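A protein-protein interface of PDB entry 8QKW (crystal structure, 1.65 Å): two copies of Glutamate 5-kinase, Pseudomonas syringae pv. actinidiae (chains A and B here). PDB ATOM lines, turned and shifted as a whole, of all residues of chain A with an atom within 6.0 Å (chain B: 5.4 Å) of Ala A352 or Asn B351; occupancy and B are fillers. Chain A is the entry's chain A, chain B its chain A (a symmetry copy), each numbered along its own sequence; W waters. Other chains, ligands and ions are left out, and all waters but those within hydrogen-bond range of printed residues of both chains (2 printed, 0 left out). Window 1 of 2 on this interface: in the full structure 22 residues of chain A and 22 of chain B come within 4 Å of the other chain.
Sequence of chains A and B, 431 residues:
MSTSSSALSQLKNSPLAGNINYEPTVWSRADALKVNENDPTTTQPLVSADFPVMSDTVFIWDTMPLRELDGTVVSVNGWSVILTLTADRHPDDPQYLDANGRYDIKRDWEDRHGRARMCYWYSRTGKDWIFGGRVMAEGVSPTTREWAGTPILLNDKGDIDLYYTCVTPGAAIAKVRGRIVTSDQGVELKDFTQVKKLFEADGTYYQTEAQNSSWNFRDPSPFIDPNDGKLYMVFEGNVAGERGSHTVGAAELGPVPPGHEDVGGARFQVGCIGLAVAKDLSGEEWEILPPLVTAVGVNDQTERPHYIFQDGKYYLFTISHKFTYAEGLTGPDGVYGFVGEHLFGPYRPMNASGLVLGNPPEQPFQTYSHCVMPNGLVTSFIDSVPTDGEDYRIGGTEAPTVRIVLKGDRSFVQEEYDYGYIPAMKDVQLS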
ATOM      1  N   TRP A  27     -18.286  28.967 -27.696  1.00  0.00           N
ATOM      2  CA  TRP A  27     -19.606  29.465 -27.255  1.00  0.00           C
ATOM      3  C   TRP A  27     -20.610  28.933 -28.262  1.00  0.00           C
ATOM      4  O   TRP A  27     -20.544  29.297 -29.453  1.00  0.00           O
ATOM      5  CB  TRP A  27     -19.544  30.993 -27.306  1.00  0.00           C
ATOM      6  CG  TRP A  27     -20.801  31.683 -26.772  1.00  0.00           C
ATOM      7  CD1 TRP A  27     -21.620  31.240 -25.770  1.00  0.00           C
ATOM      8  CD2 TRP A  27     -21.291  32.992 -27.150  1.00  0.00           C
ATOM      9  NE1 TRP A  27     -22.640  32.145 -25.528  1.00  0.00           N
ATOM     10  CE2 TRP A  27     -22.450  33.238 -26.351  1.00  0.00           C
ATOM     11  CE3 TRP A  27     -20.878  33.973 -28.074  1.00  0.00           C
ATOM     12  CZ2 TRP A  27     -23.224  34.394 -26.467  1.00  0.00           C
ATOM     13  CZ3 TRP A  27     -21.616  35.145 -28.147  1.00  0.00           C
ATOM     14  CH2 TRP A  27     -22.787  35.340 -27.378  1.00  0.00           C
ATOM     15  N   ASP A  31     -25.681  27.270 -25.848  1.00  0.00           N
ATOM     16  CA  ASP A  31     -25.438  28.293 -24.818  1.00  0.00           C
ATOM     17  C   ASP A  31     -26.228  29.578 -25.113  1.00  0.00           C
ATOM     18  O   ASP A  31     -26.857  30.174 -24.224  1.00  0.00           O
ATOM     19  CB  ASP A  31     -23.967  28.696 -24.741  1.00  0.00           C
ATOM     20  CG  ASP A  31     -22.972  27.582 -24.388  1.00  0.00           C
ATOM     21  OD1 ASP A  31     -23.319  26.670 -23.578  1.00  0.00           O
ATOM     22  OD2 ASP A  31     -21.789  27.709 -24.836  1.00  0.00           O
ATOM     23  N   ALA A  32     -26.151  30.010 -26.390  1.00  0.00           N
ATOM     24  CA  ALA A  32     -26.752  31.281 -26.777  1.00  0.00           C
ATOM     25  C   ALA A  32     -28.285  31.206 -26.718  1.00  0.00           C
ATOM     26  O   ALA A  32     -28.941  32.236 -26.519  1.00  0.00           O
ATOM     27  CB  ALA A  32     -26.266  31.708 -28.177  1.00  0.00           C
ATOM     28  N   LYS A  34     -29.839  30.225 -24.268  1.00  0.00           N
ATOM     29  CA  LYS A  34     -30.167  30.616 -22.899  1.00  0.00           C
ATOM     30  C   LYS A  34     -30.170  32.139 -22.680  1.00  0.00           C
ATOM     31  O   LYS A  34     -30.550  32.599 -21.603  1.00  0.00           O
ATOM     32  CB  LYS A  34     -29.182  29.994 -21.889  1.00  0.00           C
ATOM     33  CG  LYS A  34     -29.111  28.469 -21.879  1.00  0.00           C
ATOM     34  CD  LYS A  34     -28.111  28.009 -20.780  1.00  0.00           C
ATOM     35  CE  LYS A  34     -28.133  26.497 -20.524  1.00  0.00           C
ATOM     36  NZ  LYS A  34     -29.460  25.926 -20.107  1.00  0.00           N
ATOM     37  N   PRO A 349     -19.379  30.145 -20.020  1.00  0.00           N
ATOM     38  CA  PRO A 349     -20.162  31.377 -20.278  1.00  0.00           C
ATOM     39  C   PRO A 349     -20.733  31.924 -18.958  1.00  0.00           C
ATOM     40  O   PRO A 349     -21.327  31.202 -18.142  1.00  0.00           O
ATOM     41  CB  PRO A 349     -21.310  30.928 -21.225  1.00  0.00           C
ATOM     42  CG  PRO A 349     -21.370  29.390 -21.005  1.00  0.00           C
ATOM     43  CD  PRO A 349     -20.021  28.902 -20.533  1.00  0.00           C
ATOM     44  N   MET A 350     -20.540  33.226 -18.738  1.00  0.00           N
ATOM     45  CA  MET A 350     -21.102  33.902 -17.579  1.00  0.00           C
ATOM     46  C   MET A 350     -22.623  33.753 -17.552  1.00  0.00           C
ATOM     47  O   MET A 350     -23.248  33.917 -18.587  1.00  0.00           O
ATOM     48  CB  MET A 350     -20.744  35.387 -17.606  1.00  0.00           C
ATOM     49  CG  MET A 350     -19.282  35.592 -17.198  1.00  0.00           C
ATOM     50  SD  MET A 350     -18.913  35.215 -15.449  1.00  0.00           S
ATOM     51  CE  MET A 350     -19.600  36.678 -14.688  1.00  0.00           C
ATOM     52  N   ASN A 351     -23.184  33.514 -16.343  1.00  0.00           N
ATOM     53  CA  ASN A 351     -24.654  33.467 -16.225  1.00  0.00           C
ATOM     54  C   ASN A 351     -25.249  32.412 -17.158  1.00  0.00           C
ATOM     55  O   ASN A 351     -26.407  32.540 -17.511  1.00  0.00           O
ATOM     56  CB  ASN A 351     -25.329  34.820 -16.521  1.00  0.00           C
ATOM     57  CG  ASN A 351     -24.841  35.899 -15.559  1.00  0.00           C
ATOM     58  OD1 ASN A 351     -24.858  35.722 -14.322  1.00  0.00           O
ATOM     59  ND2 ASN A 351     -24.366  37.013 -16.093  1.00  0.00           N
ATOM     60  N   ALA A 352     -24.453  31.392 -17.503  1.00  0.00           N
ATOM     61  CA  ALA A 352     -24.870  30.242 -18.310  1.00  0.00           C
ATOM     62  C   ALA A 352     -24.997  30.591 -19.790  1.00  0.00           C
ATOM     63  O   ALA A 352     -24.665  29.741 -20.614  1.00  0.00           O
ATOM     64  CB  ALA A 352     -26.104  29.499 -17.767  1.00  0.00           C
ATOM     65  N   SER A 353     -25.538  31.789 -20.129  1.00  0.00           N
ATOM     66  CA  SER A 353     -25.741  32.084 -21.550  1.00  0.00           C
ATOM     67  C   SER A 353     -24.544  32.828 -22.151  1.00  0.00           C
ATOM     68  O   SER A 353     -24.432  32.896 -23.380  1.00  0.00           O
ATOM     69  CB  SER A 353     -26.965  32.991 -21.686  1.00  0.00           C
ATOM     70  OG  SER A 353     -26.710  34.239 -21.001  1.00  0.00           O
ATOM     71  N   GLY A 354     -23.758  33.492 -21.276  1.00  0.00           N
ATOM     72  CA  GLY A 354     -22.733  34.433 -21.689  1.00  0.00           C
ATOM     73  C   GLY A 354     -23.122  35.901 -21.460  1.00  0.00           C
ATOM     74  O   GLY A 354     -22.256  36.769 -21.406  1.00  0.00           O
ATOM     75  N   LEU A 355     -24.439  36.203 -21.340  1.00  0.00           N
ATOM     76  CA  LEU A 355     -24.786  37.635 -21.238  1.00  0.00           C
ATOM     77  C   LEU A 355     -24.515  38.179 -19.827  1.00  0.00           C
ATOM     78  O   LEU A 355     -24.965  37.603 -18.818  1.00  0.00           O
ATOM     79  CB  LEU A 355     -26.291  37.767 -21.532  1.00  0.00           C
ATOM     80  CG  LEU A 355     -26.857  39.192 -21.388  1.00  0.00           C
ATOM     81  CD1 LEU A 355     -26.227  40.110 -22.454  1.00  0.00           C
ATOM     82  CD2 LEU A 355     -28.403  39.184 -21.469  1.00  0.00           C
ATOM     83  N   ASP A 409     -19.425  32.219 -11.356  1.00  0.00           N
ATOM     84  CA  ASP A 409     -19.626  32.320 -12.799  1.00  0.00           C
ATOM     85  C   ASP A 409     -20.846  33.192 -13.136  1.00  0.00           C
ATOM     86  O   ASP A 409     -21.451  33.038 -14.175  1.00  0.00           O
ATOM     87  CB  ASP A 409     -19.811  30.890 -13.375  1.00  0.00           C
ATOM     88  CG  ASP A 409     -18.544  30.036 -13.340  1.00  0.00           C
ATOM     89  OD1 ASP A 409     -17.536  30.467 -12.773  1.00  0.00           O
ATOM     90  OD2 ASP A 409     -18.595  28.887 -13.837  1.00  0.00           O
ATOM     91  N   THR B  42     -34.417  24.651 -21.094  1.00  0.00           N
ATOM     92  CA  THR B  42     -34.803  24.226 -19.740  1.00  0.00           C
ATOM     93  C   THR B  42     -36.319  24.133 -19.638  1.00  0.00           C
ATOM     94  O   THR B  42     -36.855  24.309 -18.565  1.00  0.00           O
ATOM     95  CB  THR B  42     -34.202  25.129 -18.641  1.00  0.00           C
ATOM     96  OG1 THR B  42     -34.610  26.496 -18.805  1.00  0.00           O
ATOM     97  CG2 THR B  42     -32.680  25.058 -18.646  1.00  0.00           C
ATOM     98  N   PRO B 349     -26.038  27.335  -8.130  1.00  0.00           N
ATOM     99  CA  PRO B 349     -27.331  27.072  -8.806  1.00  0.00           C
ATOM    100  C   PRO B 349     -27.087  26.678 -10.273  1.00  0.00           C
ATOM    101  O   PRO B 349     -26.338  27.328 -11.020  1.00  0.00           O
ATOM    102  CB  PRO B 349     -28.104  28.418  -8.724  1.00  0.00           C
ATOM    103  CG  PRO B 349     -26.979  29.458  -8.464  1.00  0.00           C
ATOM    104  CD  PRO B 349     -25.808  28.771  -7.803  1.00  0.00           C
ATOM    105  N   MET B 350     -27.725  25.583 -10.693  1.00  0.00           N
ATOM    106  CA  MET B 350     -27.664  25.142 -12.078  1.00  0.00           C
ATOM    107  C   MET B 350     -28.171  26.237 -13.017  1.00  0.00           C
ATOM    108  O   MET B 350     -29.189  26.840 -12.720  1.00  0.00           O
ATOM    109  CB  MET B 350     -28.512  23.885 -12.272  1.00  0.00           C
ATOM    110  CG  MET B 350     -27.791  22.661 -11.697  1.00  0.00           C
ATOM    111  SD  MET B 350     -26.285  22.163 -12.603  1.00  0.00           S
ATOM    112  CE  MET B 350     -27.045  21.376 -14.015  1.00  0.00           C
ATOM    113  N   ASN B 351     -27.477  26.414 -14.166  1.00  0.00           N
ATOM    114  CA  ASN B 351     -27.971  27.377 -15.168  1.00  0.00           C
ATOM    115  C   ASN B 351     -28.112  28.776 -14.565  1.00  0.00           C
ATOM    116  O   ASN B 351     -28.893  29.552 -15.085  1.00  0.00           O
ATOM    117  CB  ASN B 351     -29.324  26.971 -15.784  1.00  0.00           C
ATOM    118  CG  ASN B 351     -29.225  25.618 -16.482  1.00  0.00           C
ATOM    119  OD1 ASN B 351     -28.332  25.386 -17.324  1.00  0.00           O
ATOM    120  ND2 ASN B 351     -30.101  24.691 -16.128  1.00  0.00           N
ATOM    121  N   ALA B 352     -27.336  29.062 -13.513  1.00  0.00           N
ATOM    122  CA  ALA B 352     -27.261  30.372 -12.860  1.00  0.00           C
ATOM    123  C   ALA B 352     -28.480  30.651 -11.985  1.00  0.00           C
ATOM    124  O   ALA B 352     -28.307  31.266 -10.935  1.00  0.00           O
ATOM    125  CB  ALA B 352     -26.932  31.537 -13.811  1.00  0.00           C
ATOM    126  N   SER B 353     -29.703  30.277 -12.440  1.00  0.00           N
ATOM    127  CA  SER B 353     -30.880  30.625 -11.640  1.00  0.00           C
ATOM    128  C   SER B 353     -31.261  29.501 -10.672  1.00  0.00           C
ATOM    129  O   SER B 353     -32.038  29.743  -9.742  1.00  0.00           O
ATOM    130  CB  SER B 353     -32.062  30.841 -12.586  1.00  0.00           C
ATOM    131  OG  SER B 353     -32.344  29.606 -13.283  1.00  0.00           O
ATOM    132  N   GLY B 354     -30.821  28.265 -10.996  1.00  0.00           N
ATOM    133  CA  GLY B 354     -31.283  27.061 -10.329  1.00  0.00           C
ATOM    134  C   GLY B 354     -32.262  26.231 -11.174  1.00  0.00           C
ATOM    135  O   GLY B 354     -32.444  25.045 -10.920  1.00  0.00           O
ATOM    136  N   LEU B 355     -32.922  26.852 -12.182  1.00  0.00           N
ATOM    137  CA  LEU B 355     -33.941  26.057 -12.899  1.00  0.00           C
ATOM    138  C   LEU B 355     -33.294  25.085 -13.897  1.00  0.00           C
ATOM    139  O   LEU B 355     -32.460  25.482 -14.733  1.00  0.00           O
ATOM    140  CB  LEU B 355     -34.828  27.042 -13.681  1.00  0.00           C
ATOM    141  CG  LEU B 355     -35.905  26.383 -14.564  1.00  0.00           C
ATOM    142  CD1 LEU B 355     -36.926  25.648 -13.673  1.00  0.00           C
ATOM    143  CD2 LEU B 355     -36.582  27.429 -15.483  1.00  0.00           C
ATOM    144  N   VAL B 356     -33.794  23.821 -13.850  1.00  0.00           N
ATOM    145  CA  VAL B 356     -33.261  22.766 -14.709  1.00  0.00           C
ATOM    146  C   VAL B 356     -34.328  22.391 -15.744  1.00  0.00           C
ATOM    147  O   VAL B 356     -34.012  22.318 -16.950  1.00  0.00           O
ATOM    148  CB  VAL B 356     -32.849  21.535 -13.873  1.00  0.00           C
ATOM    149  CG1 VAL B 356     -32.622  20.273 -14.723  1.00  0.00           C
ATOM    150  CG2 VAL B 356     -31.596  21.844 -13.027  1.00  0.00           C
ATOM    151  N   ASP B 409     -21.932  23.366 -14.968  1.00  0.00           N
ATOM    152  CA  ASP B 409     -22.994  23.855 -14.094  1.00  0.00           C
ATOM    153  C   ASP B 409     -24.279  24.152 -14.883  1.00  0.00           C
ATOM    154  O   ASP B 409     -25.083  24.964 -14.478  1.00  0.00           O
ATOM    155  CB  ASP B 409     -22.494  25.138 -13.376  1.00  0.00           C
ATOM    156  CG  ASP B 409     -21.394  24.887 -12.346  1.00  0.00           C
ATOM    157  OD1 ASP B 409     -20.907  23.758 -12.241  1.00  0.00           O
ATOM    158  OD2 ASP B 409     -20.974  25.864 -11.684  1.00  0.00           O
ATOM    159  N   ARG B 410     -24.454  23.568 -16.080  1.00  0.00           N
ATOM    160  CA  ARG B 410     -25.591  23.881 -16.923  1.00  0.00           C
ATOM    161  C   ARG B 410     -26.248  22.575 -17.353  1.00  0.00           C
ATOM    162  O   ARG B 410     -25.643  21.509 -17.297  1.00  0.00           O
ATOM    163  CB  ARG B 410     -25.129  24.617 -18.204  1.00  0.00           C
ATOM    164  CG  ARG B 410     -24.484  25.992 -17.953  1.00  0.00           C
ATOM    165  CD  ARG B 410     -22.951  26.038 -18.136  1.00  0.00           C
ATOM    166  NE  ARG B 410     -22.702  25.872 -19.583  1.00  0.00           N
ATOM    167  CZ  ARG B 410     -21.536  25.483 -20.107  1.00  0.00           C
ATOM    168  NH1 ARG B 410     -20.513  25.142 -19.325  1.00  0.00           N
ATOM    169  NH2 ARG B 410     -21.365  25.571 -21.421  1.00  0.00           N
ATOM    170  N   SER B 411     -27.519  22.695 -17.744  1.00  0.00           N
ATOM    171  CA  SER B 411     -28.237  21.537 -18.284  1.00  0.00           C
ATOM    172  C   SER B 411     -28.968  21.931 -19.552  1.00  0.00           C
ATOM    173  O   SER B 411     -29.271  23.100 -19.785  1.00  0.00           O
ATOM    174  CB  SER B 411     -29.254  20.986 -17.259  1.00  0.00           C
ATOM    175  OG  SER B 411     -30.294  21.949 -17.065  1.00  0.00           O
HETATM  176  O   HOH W   1     -18.453  26.754 -12.161  1.00  0.00           O
HETATM  177  O   HOH W   2     -24.536  27.124 -21.273  1.00  0.00           O
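The guanidinium group (NH2) of Arg B410 lies within salt-bridge range of the side-chain carboxylate (OD1) of Asp A31 (3.1 Å). The side-chain amino group (NZ) of Lys A34 lies within hydrogen-bond range of the side-chain amide oxygen (OD1) of Asn B351 (3.1 Å). The backbone carbonyl oxygen of Ser B411 lies within hydrogen-bond range of the side-chain amino group of Lys A34 (2.9 Å).
The side-chain amide nitrogen (ND2) of Asn A351 sits at hydrogen-bond distance from the backbone carbonyl oxygen (O) of Leu A355 (2.9 Å). The backbone NH (N) of Asn A351 is in hydrogen-bond range of the backbone carbonyl oxygen (O) of Asp A409 (2.8 Å). ND2 of Asn B351 is in hydrogen-bond range of O of Leu B355 (2.9 Å). The backbone NH of Asn B351 lies within hydrogen-bond range of the backbone carbonyl oxygen of Asp B409, at 2.8 Å. OD1 of Asn B351 is in hydrogen-bond range of N of Ser B411 (2.8 Å).
Among the printed residues, pairs that only touch across the chains: Lys A34 with Thr B42 (3.6 Å), Pro A349 with Arg B410 (3.7 Å), Asn A351 with Ala B352 (3.8 Å), Ala A352 with Asn B351 (3.8 Å) and Ala A352 with Arg B410 (3.9 Å).
Asn B351 touches two residues of chain A. Of the printed residues of chain A, Arg B410 touches Asp A31 (3.1 Å), Pro A349 (3.7 Å) and Ala A352 (3.9 Å). Of the printed residues of chain B, Lys A34 touches Thr B42 (3.6 Å), Asn B351 (3.1 Å) and Ser B411 (2.9 Å). Met A350 touches none of the printed residues of chain B. The nearest printed residue of chain B that does not touch Lys A34 is Arg B410 (4.2 Å).
Of the 12 printed residues of chain A, 5 touch a printed residue of chain B. Printed residues of chain A that touch a printed residue of chain B: Asp A31, Lys A34, Pro A349, Asn A351 and Ala A352. Hydrophobic or aromatic side chains of chain A that line the printed part of chain B: Pro A349 and Ala A352. Of the 12 printed residues of chain B, 5 touch a printed residue of chain A. Among the printed residues, Asp or Glu carboxylates within 4 Å of a Lys or Arg side-chain nitrogen of the other chain: Asp A31 with Arg B410.
Asn A351 touches Ala B352, and with the chains exchanged Ala A352 touches Asn B351.
Water W2 lies within hydrogen-bond range of the side-chain carboxylate of Asp A31 (2.6 Å), the backbone carbonyl oxygen of Ala A352 (2.7 Å) and the guanidinium group of Arg B410 (2.8 Å). Water W1 lies within hydrogen-bond range of OD2 of Asp A409 and OD2 of Asp B409.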
